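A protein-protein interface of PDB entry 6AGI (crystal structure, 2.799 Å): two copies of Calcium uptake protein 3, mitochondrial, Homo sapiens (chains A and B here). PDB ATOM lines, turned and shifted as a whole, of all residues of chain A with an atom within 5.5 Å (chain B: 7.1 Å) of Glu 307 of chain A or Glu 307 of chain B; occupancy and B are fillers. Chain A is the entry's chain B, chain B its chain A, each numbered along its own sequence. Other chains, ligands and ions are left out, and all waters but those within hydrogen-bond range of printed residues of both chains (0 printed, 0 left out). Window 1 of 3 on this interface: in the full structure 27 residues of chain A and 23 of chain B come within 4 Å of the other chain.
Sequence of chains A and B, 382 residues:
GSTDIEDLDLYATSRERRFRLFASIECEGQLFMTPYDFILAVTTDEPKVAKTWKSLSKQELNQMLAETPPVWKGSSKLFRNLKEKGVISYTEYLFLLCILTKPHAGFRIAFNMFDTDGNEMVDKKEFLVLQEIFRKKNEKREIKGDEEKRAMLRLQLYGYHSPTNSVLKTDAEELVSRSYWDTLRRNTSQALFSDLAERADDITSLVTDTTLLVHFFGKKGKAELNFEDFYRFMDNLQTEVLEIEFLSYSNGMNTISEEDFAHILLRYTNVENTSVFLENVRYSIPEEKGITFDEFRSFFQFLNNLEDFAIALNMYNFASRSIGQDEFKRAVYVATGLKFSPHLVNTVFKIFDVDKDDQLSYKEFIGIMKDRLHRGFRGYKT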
ATOM      1  N   LEU A 303      14.248 -11.504   2.168  1.00  0.00           N
ATOM      2  CA  LEU A 303      13.497 -10.269   1.923  1.00  0.00           C
ATOM      3  C   LEU A 303      13.506  -9.373   3.137  1.00  0.00           C
ATOM      4  O   LEU A 303      13.452  -8.145   2.991  1.00  0.00           O
ATOM      5  CB  LEU A 303      12.044 -10.514   1.524  1.00  0.00           C
ATOM      6  CG  LEU A 303      11.841 -11.031   0.119  1.00  0.00           C
ATOM      7  CD1 LEU A 303      10.359 -11.086  -0.258  1.00  0.00           C
ATOM      8  CD2 LEU A 303      12.683 -10.201  -0.835  1.00  0.00           C
ATOM      9  N   ASN A 304      13.614  -9.947   4.334  1.00  0.00           N
ATOM     10  CA  ASN A 304      13.703  -9.010   5.436  1.00  0.00           C
ATOM     11  C   ASN A 304      15.105  -8.460   5.617  1.00  0.00           C
ATOM     12  O   ASN A 304      15.266  -7.452   6.311  1.00  0.00           O
ATOM     13  CB  ASN A 304      13.162  -9.624   6.730  1.00  0.00           C
ATOM     14  CG  ASN A 304      11.653  -9.615   6.758  1.00  0.00           C
ATOM     15  OD1 ASN A 304      11.024  -8.988   5.916  1.00  0.00           O
ATOM     16  ND2 ASN A 304      11.068 -10.278   7.721  1.00  0.00           N
ATOM     17  N   ASN A 305      16.104  -9.037   4.951  1.00  0.00           N
ATOM     18  CA  ASN A 305      17.465  -8.511   4.993  1.00  0.00           C
ATOM     19  C   ASN A 305      17.819  -7.811   3.673  1.00  0.00           C
ATOM     20  O   ASN A 305      18.991  -7.752   3.239  1.00  0.00           O
ATOM     21  CB  ASN A 305      18.426  -9.648   5.298  1.00  0.00           C
ATOM     22  CG  ASN A 305      18.731  -9.779   6.761  1.00  0.00           C
ATOM     23  OD1 ASN A 305      18.376 -10.782   7.400  1.00  0.00           O
ATOM     24  ND2 ASN A 305      19.360  -8.754   7.322  1.00  0.00           N
ATOM     25  N   LEU A 306      16.793  -7.285   3.006  1.00  0.00           N
ATOM     26  CA  LEU A 306      17.023  -6.752   1.674  1.00  0.00           C
ATOM     27  C   LEU A 306      18.005  -5.588   1.660  1.00  0.00           C
ATOM     28  O   LEU A 306      18.696  -5.401   0.651  1.00  0.00           O
ATOM     29  CB  LEU A 306      15.703  -6.323   1.036  1.00  0.00           C
ATOM     30  CG  LEU A 306      15.883  -6.279  -0.489  1.00  0.00           C
ATOM     31  CD1 LEU A 306      15.976  -7.672  -1.063  1.00  0.00           C
ATOM     32  CD2 LEU A 306      14.763  -5.510  -1.157  1.00  0.00           C
ATOM     33  N   GLU A 307      18.002  -4.790   2.723  1.00  0.00           N
ATOM     34  CA  GLU A 307      18.869  -3.624   2.815  1.00  0.00           C
ATOM     35  C   GLU A 307      20.304  -4.075   2.680  1.00  0.00           C
ATOM     36  O   GLU A 307      21.019  -3.665   1.766  1.00  0.00           O
ATOM     37  CB  GLU A 307      18.663  -2.904   4.149  1.00  0.00           C
ATOM     38  CG  GLU A 307      17.441  -2.002   4.185  1.00  0.00           C
ATOM     39  CD  GLU A 307      16.149  -2.778   4.342  1.00  0.00           C
ATOM     40  OE1 GLU A 307      16.205  -4.025   4.394  1.00  0.00           O
ATOM     41  OE2 GLU A 307      15.076  -2.142   4.414  1.00  0.00           O
ATOM     42  N   ASP A 308      20.719  -4.932   3.601  1.00  0.00           N
ATOM     43  CA  ASP A 308      22.077  -5.465   3.576  1.00  0.00           C
ATOM     44  C   ASP A 308      22.404  -5.970   2.180  1.00  0.00           C
ATOM     45  O   ASP A 308      23.508  -5.726   1.662  1.00  0.00           O
ATOM     46  CB  ASP A 308      22.251  -6.601   4.591  1.00  0.00           C
ATOM     47  CG  ASP A 308      22.338  -6.104   6.043  1.00  0.00           C
ATOM     48  OD1 ASP A 308      21.809  -4.995   6.319  1.00  0.00           O
ATOM     49  OD2 ASP A 308      22.971  -6.767   6.900  1.00  0.00           O
ATOM     50  N   PHE A 309      21.423  -6.587   1.506  1.00  0.00           N
ATOM     51  CA  PHE A 309      21.680  -7.014   0.126  1.00  0.00           C
ATOM     52  C   PHE A 309      21.984  -5.824  -0.788  1.00  0.00           C
ATOM     53  O   PHE A 309      22.898  -5.888  -1.633  1.00  0.00           O
ATOM     54  CB  PHE A 309      20.491  -7.800  -0.415  1.00  0.00           C
ATOM     55  CG  PHE A 309      20.777  -8.548  -1.701  1.00  0.00           C
ATOM     56  CD1 PHE A 309      21.674  -9.609  -1.730  1.00  0.00           C
ATOM     57  CD2 PHE A 309      20.119  -8.199  -2.877  1.00  0.00           C
ATOM     58  CE1 PHE A 309      21.921 -10.300  -2.913  1.00  0.00           C
ATOM     59  CE2 PHE A 309      20.353  -8.896  -4.063  1.00  0.00           C
ATOM     60  CZ  PHE A 309      21.259  -9.949  -4.080  1.00  0.00           C
ATOM     61  N   ALA A 310      21.234  -4.726  -0.643  1.00  0.00           N
ATOM     62  CA  ALA A 310      21.487  -3.576  -1.507  1.00  0.00           C
ATOM     63  C   ALA A 310      22.892  -3.040  -1.287  1.00  0.00           C
ATOM     64  O   ALA A 310      23.616  -2.773  -2.258  1.00  0.00           O
ATOM     65  CB  ALA A 310      20.451  -2.480  -1.259  1.00  0.00           C
ATOM     66  N   ILE A 311      23.315  -2.930  -0.016  1.00  0.00           N
ATOM     67  CA  ILE A 311      24.702  -2.553   0.273  1.00  0.00           C
ATOM     68  C   ILE A 311      25.679  -3.461  -0.473  1.00  0.00           C
ATOM     69  O   ILE A 311      26.616  -2.998  -1.124  1.00  0.00           O
ATOM     70  CB  ILE A 311      24.973  -2.586   1.788  1.00  0.00           C
ATOM     71  CG1 ILE A 311      24.410  -1.341   2.475  1.00  0.00           C
ATOM     72  CG2 ILE A 311      26.461  -2.786   2.076  1.00  0.00           C
ATOM     73  CD1 ILE A 311      24.392  -1.473   3.976  1.00  0.00           C
ATOM     74  N   ALA A 312      25.470  -4.769  -0.389  1.00  0.00           N
ATOM     75  CA  ALA A 312      26.387  -5.696  -1.036  1.00  0.00           C
ATOM     76  C   ALA A 312      26.471  -5.458  -2.542  1.00  0.00           C
ATOM     77  O   ALA A 312      27.558  -5.545  -3.122  1.00  0.00           O
ATOM     78  CB  ALA A 312      25.971  -7.136  -0.737  1.00  0.00           C
ATOM     79  N   PRO B 103      27.624   2.307   5.334  1.00  0.00           N
ATOM     80  CA  PRO B 103      27.791   2.407   6.782  1.00  0.00           C
ATOM     81  C   PRO B 103      28.897   1.472   7.238  1.00  0.00           C
ATOM     82  O   PRO B 103      29.252   0.508   6.553  1.00  0.00           O
ATOM     83  CB  PRO B 103      26.427   1.949   7.320  1.00  0.00           C
ATOM     84  CG  PRO B 103      25.983   0.942   6.336  1.00  0.00           C
ATOM     85  CD  PRO B 103      26.511   1.402   4.981  1.00  0.00           C
ATOM     86  N   PHE B 302      25.014   8.735  10.635  1.00  0.00           N
ATOM     87  CA  PHE B 302      23.638   8.291  10.831  1.00  0.00           C
ATOM     88  C   PHE B 302      22.909   8.138   9.496  1.00  0.00           C
ATOM     89  O   PHE B 302      22.213   7.138   9.276  1.00  0.00           O
ATOM     90  CB  PHE B 302      22.909   9.316  11.703  1.00  0.00           C
ATOM     91  CG  PHE B 302      21.417   9.175  11.718  1.00  0.00           C
ATOM     92  CD1 PHE B 302      20.814   8.032  12.237  1.00  0.00           C
ATOM     93  CD2 PHE B 302      20.615  10.217  11.309  1.00  0.00           C
ATOM     94  CE1 PHE B 302      19.425   7.909  12.294  1.00  0.00           C
ATOM     95  CE2 PHE B 302      19.224  10.106  11.356  1.00  0.00           C
ATOM     96  CZ  PHE B 302      18.625   8.946  11.853  1.00  0.00           C
ATOM     97  N   LEU B 303      23.121   9.075   8.558  1.00  0.00           N
ATOM     98  CA  LEU B 303      22.429   8.961   7.272  1.00  0.00           C
ATOM     99  C   LEU B 303      22.805   7.704   6.488  1.00  0.00           C
ATOM    100  O   LEU B 303      22.015   7.241   5.650  1.00  0.00           O
ATOM    101  CB  LEU B 303      22.705  10.167   6.381  1.00  0.00           C
ATOM    102  CG  LEU B 303      22.030  11.480   6.699  1.00  0.00           C
ATOM    103  CD1 LEU B 303      22.407  12.476   5.604  1.00  0.00           C
ATOM    104  CD2 LEU B 303      20.556  11.224   6.742  1.00  0.00           C
ATOM    105  N   ASN B 304      23.997   7.152   6.704  1.00  0.00           N
ATOM    106  CA  ASN B 304      24.305   5.930   5.978  1.00  0.00           C
ATOM    107  C   ASN B 304      23.733   4.701   6.655  1.00  0.00           C
ATOM    108  O   ASN B 304      23.746   3.623   6.059  1.00  0.00           O
ATOM    109  CB  ASN B 304      25.810   5.780   5.788  1.00  0.00           C
ATOM    110  CG  ASN B 304      26.356   6.703   4.714  1.00  0.00           C
ATOM    111  OD1 ASN B 304      25.595   7.345   3.995  1.00  0.00           O
ATOM    112  ND2 ASN B 304      27.681   6.691   4.532  1.00  0.00           N
ATOM    113  N   ASN B 305      23.238   4.854   7.880  1.00  0.00           N
ATOM    114  CA  ASN B 305      22.611   3.799   8.669  1.00  0.00           C
ATOM    115  C   ASN B 305      21.111   3.996   8.820  1.00  0.00           C
ATOM    116  O   ASN B 305      20.512   3.521   9.788  1.00  0.00           O
ATOM    117  CB  ASN B 305      23.263   3.719  10.050  1.00  0.00           C
ATOM    118  CG  ASN B 305      24.078   2.488  10.225  1.00  0.00           C
ATOM    119  OD1 ASN B 305      23.573   1.382  10.037  1.00  0.00           O
ATOM    120  ND2 ASN B 305      25.350   2.655  10.559  1.00  0.00           N
ATOM    121  N   LEU B 306      20.492   4.686   7.869  1.00  0.00           N
ATOM    122  CA  LEU B 306      19.086   5.032   8.004  1.00  0.00           C
ATOM    123  C   LEU B 306      18.175   3.822   8.050  1.00  0.00           C
ATOM    124  O   LEU B 306      17.070   3.922   8.581  1.00  0.00           O
ATOM    125  CB  LEU B 306      18.657   5.935   6.858  1.00  0.00           C
ATOM    126  CG  LEU B 306      18.589   7.414   7.190  1.00  0.00           C
ATOM    127  CD1 LEU B 306      18.098   8.133   5.950  1.00  0.00           C
ATOM    128  CD2 LEU B 306      17.644   7.644   8.362  1.00  0.00           C
ATOM    129  N   GLU B 307      18.594   2.677   7.527  1.00  0.00           N
ATOM    130  CA  GLU B 307      17.634   1.585   7.446  1.00  0.00           C
ATOM    131  C   GLU B 307      17.530   0.859   8.782  1.00  0.00           C
ATOM    132  O   GLU B 307      16.439   0.400   9.156  1.00  0.00           O
ATOM    133  CB  GLU B 307      18.031   0.640   6.297  1.00  0.00           C
ATOM    134  CG  GLU B 307      18.208   1.377   4.937  1.00  0.00           C
ATOM    135  CD  GLU B 307      19.598   2.035   4.783  1.00  0.00           C
ATOM    136  OE1 GLU B 307      20.527   1.700   5.559  1.00  0.00           O
ATOM    137  OE2 GLU B 307      19.761   2.911   3.906  1.00  0.00           O
ATOM    138  N   ASP B 308      18.624   0.819   9.551  1.00  0.00           N
ATOM    139  CA  ASP B 308      18.520   0.453  10.960  1.00  0.00           C
ATOM    140  C   ASP B 308      17.643   1.445  11.725  1.00  0.00           C
ATOM    141  O   ASP B 308      16.864   1.054  12.614  1.00  0.00           O
ATOM    142  CB  ASP B 308      19.921   0.354  11.570  1.00  0.00           C
ATOM    143  CG  ASP B 308      20.612  -0.992  11.271  1.00  0.00           C
ATOM    144  OD1 ASP B 308      20.161  -1.702  10.344  1.00  0.00           O
ATOM    145  OD2 ASP B 308      21.630  -1.326  11.949  1.00  0.00           O
ATOM    146  N   PHE B 309      17.731   2.736  11.383  1.00  0.00           N
ATOM    147  CA  PHE B 309      16.858   3.711  12.038  1.00  0.00           C
ATOM    148  C   PHE B 309      15.391   3.461  11.728  1.00  0.00           C
ATOM    149  O   PHE B 309      14.520   3.554  12.614  1.00  0.00           O
ATOM    150  CB  PHE B 309      17.244   5.125  11.636  1.00  0.00           C
ATOM    151  CG  PHE B 309      16.593   6.153  12.478  1.00  0.00           C
ATOM    152  CD1 PHE B 309      16.868   6.179  13.832  1.00  0.00           C
ATOM    153  CD2 PHE B 309      15.713   7.094  11.945  1.00  0.00           C
ATOM    154  CE1 PHE B 309      16.287   7.120  14.649  1.00  0.00           C
ATOM    155  CE2 PHE B 309      15.128   8.057  12.759  1.00  0.00           C
ATOM    156  CZ  PHE B 309      15.406   8.066  14.109  1.00  0.00           C
ATOM    157  N   ALA B 310      15.087   3.153  10.476  1.00  0.00           N
ATOM    158  CA  ALA B 310      13.705   2.878  10.148  1.00  0.00           C
ATOM    159  C   ALA B 310      13.226   1.637  10.889  1.00  0.00           C
ATOM    160  O   ALA B 310      12.109   1.624  11.428  1.00  0.00           O
ATOM    161  CB  ALA B 310      13.545   2.751   8.638  1.00  0.00           C
ATOM    162  N   ILE B 311      14.080   0.600  10.972  1.00  0.00           N
ATOM    163  CA  ILE B 311      13.729  -0.573  11.778  1.00  0.00           C
ATOM    164  C   ILE B 311      13.351  -0.144  13.196  1.00  0.00           C
ATOM    165  O   ILE B 311      12.280  -0.491  13.707  1.00  0.00           O
ATOM    166  CB  ILE B 311      14.879  -1.595  11.792  1.00  0.00           C
ATOM    167  CG1 ILE B 311      14.981  -2.326  10.450  1.00  0.00           C
ATOM    168  CG2 ILE B 311      14.641  -2.642  12.868  1.00  0.00           C
ATOM    169  CD1 ILE B 311      16.271  -3.156  10.283  1.00  0.00           C
ATOM    170  N   ALA B 312      14.193   0.680  13.821  1.00  0.00           N
ATOM    171  CA  ALA B 312      13.904   1.114  15.187  1.00  0.00           C
ATOM    172  C   ALA B 312      12.547   1.791  15.285  1.00  0.00           C
ATOM    173  O   ALA B 312      11.787   1.515  16.216  1.00  0.00           O
ATOM    174  CB  ALA B 312      14.985   2.069  15.698  1.00  0.00           C
ATOM    175  N   LEU B 313      12.209   2.661  14.334  1.00  0.00           N
ATOM    176  CA  LEU B 313      10.976   3.434  14.450  1.00  0.00           C
ATOM    177  C   LEU B 313       9.785   2.766  13.767  1.00  0.00           C
ATOM    178  O   LEU B 313       8.709   3.384  13.639  1.00  0.00           O
ATOM    179  CB  LEU B 313      11.197   4.826  13.868  1.00  0.00           C
ATOM    180  CG  LEU B 313      12.018   5.795  14.714  1.00  0.00           C
ATOM    181  CD1 LEU B 313      11.938   7.167  14.075  1.00  0.00           C
ATOM    182  CD2 LEU B 313      11.515   5.818  16.171  1.00  0.00           C
ATOM    183  N   ALA B 335      19.436   2.345  17.538  1.00  0.00           N
ATOM    184  CA  ALA B 335      19.492   1.900  16.157  1.00  0.00           C
ATOM    185  C   ALA B 335      20.914   1.809  15.649  1.00  0.00           C
ATOM    186  O   ALA B 335      21.302   0.800  15.057  1.00  0.00           O
ATOM    187  CB  ALA B 335      18.688   2.852  15.279  1.00  0.00           C
ATOM    188  N   LYS B 370      16.824  10.683   0.317  1.00  0.00           N
ATOM    189  CA  LYS B 370      17.051   9.960  -0.923  1.00  0.00           C
ATOM    190  C   LYS B 370      17.755   8.646  -0.611  1.00  0.00           C
ATOM    191  O   LYS B 370      18.526   8.547   0.349  1.00  0.00           O
ATOM    192  CB  LYS B 370      17.926  10.783  -1.878  1.00  0.00           C
ATOM    193  CG  LYS B 370      17.264  12.010  -2.490  1.00  0.00           C
ATOM    194  CD  LYS B 370      18.313  13.018  -2.966  1.00  0.00           C
ATOM    195  CE  LYS B 370      19.086  12.496  -4.179  1.00  0.00           C
ATOM    196  NZ  LYS B 370      18.943  13.374  -5.376  1.00  0.00           N
ATOM    197  N   ASP B 371      17.467   7.618  -1.407  1.00  0.00           N
ATOM    198  CA  ASP B 371      18.236   6.383  -1.275  1.00  0.00           C
ATOM    199  C   ASP B 371      19.477   6.541  -2.152  1.00  0.00           C
ATOM    200  O   ASP B 371      19.596   5.983  -3.250  1.00  0.00           O
ATOM    201  CB  ASP B 371      17.398   5.172  -1.662  1.00  0.00           C
ATOM    202  N   ARG B 372      20.440   7.298  -1.597  1.00  0.00           N
ATOM    203  CA  ARG B 372      21.807   7.466  -2.086  1.00  0.00           C
ATOM    204  C   ARG B 372      21.866   7.542  -3.611  1.00  0.00           C
ATOM    205  O   ARG B 372      22.728   6.916  -4.238  1.00  0.00           O
ATOM    206  CB  ARG B 372      22.690   6.326  -1.559  1.00  0.00           C
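Among the printed residues, merely in contact across the chains: Glu 307 of chain A with Glu 307 of chain B (3.4 Å) and Ile 311 of chain A with Pro 103 of chain B (3.7 Å).
Glu 307 of chain A touches just one residue of chain B: Glu 307.
Glu 307 of chain B touches just one residue of chain A: Glu 307.
Of the printed residues of chain A, Pro 103 of chain B touches Ile 311 (3.7 Å).
Printed residues of chain B within 4 Å of Ile 311 of chain A: Pro 103 (3.7 Å).
Leu 303 of chain A touches none of the printed residues of chain B.
The nearest residue of chain B that does not touch Glu 307 of chain A is Ile 311 of chain B (6.0 Å).
The nearest residue of chain A that does not touch Glu 307 of chain B is Ile 311 of chain A (5.2 Å).
The nearest printed residue of chain B that does not touch Ile 311 of chain A is Glu 307 of chain B (5.2 Å).
Printed residues of chain B that touch a printed residue of chain A: Pro 103 and Glu 307.
Hydrophobic or aromatic side chains of chain B within 4 Å of the printed part of chain A: Pro 103.
Printed residues of chain A that touch a printed residue of chain B: Glu 307 and Ile 311.
Hydrophobic or aromatic side chains of chain A that line the printed part of chain B: Ile 311.
Among the printed residues, 2 pairs touch across the chains.
Glu 307 of chain A touches its own counterpart, Glu 307 of chain B.
10 positions are printed for both chains.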
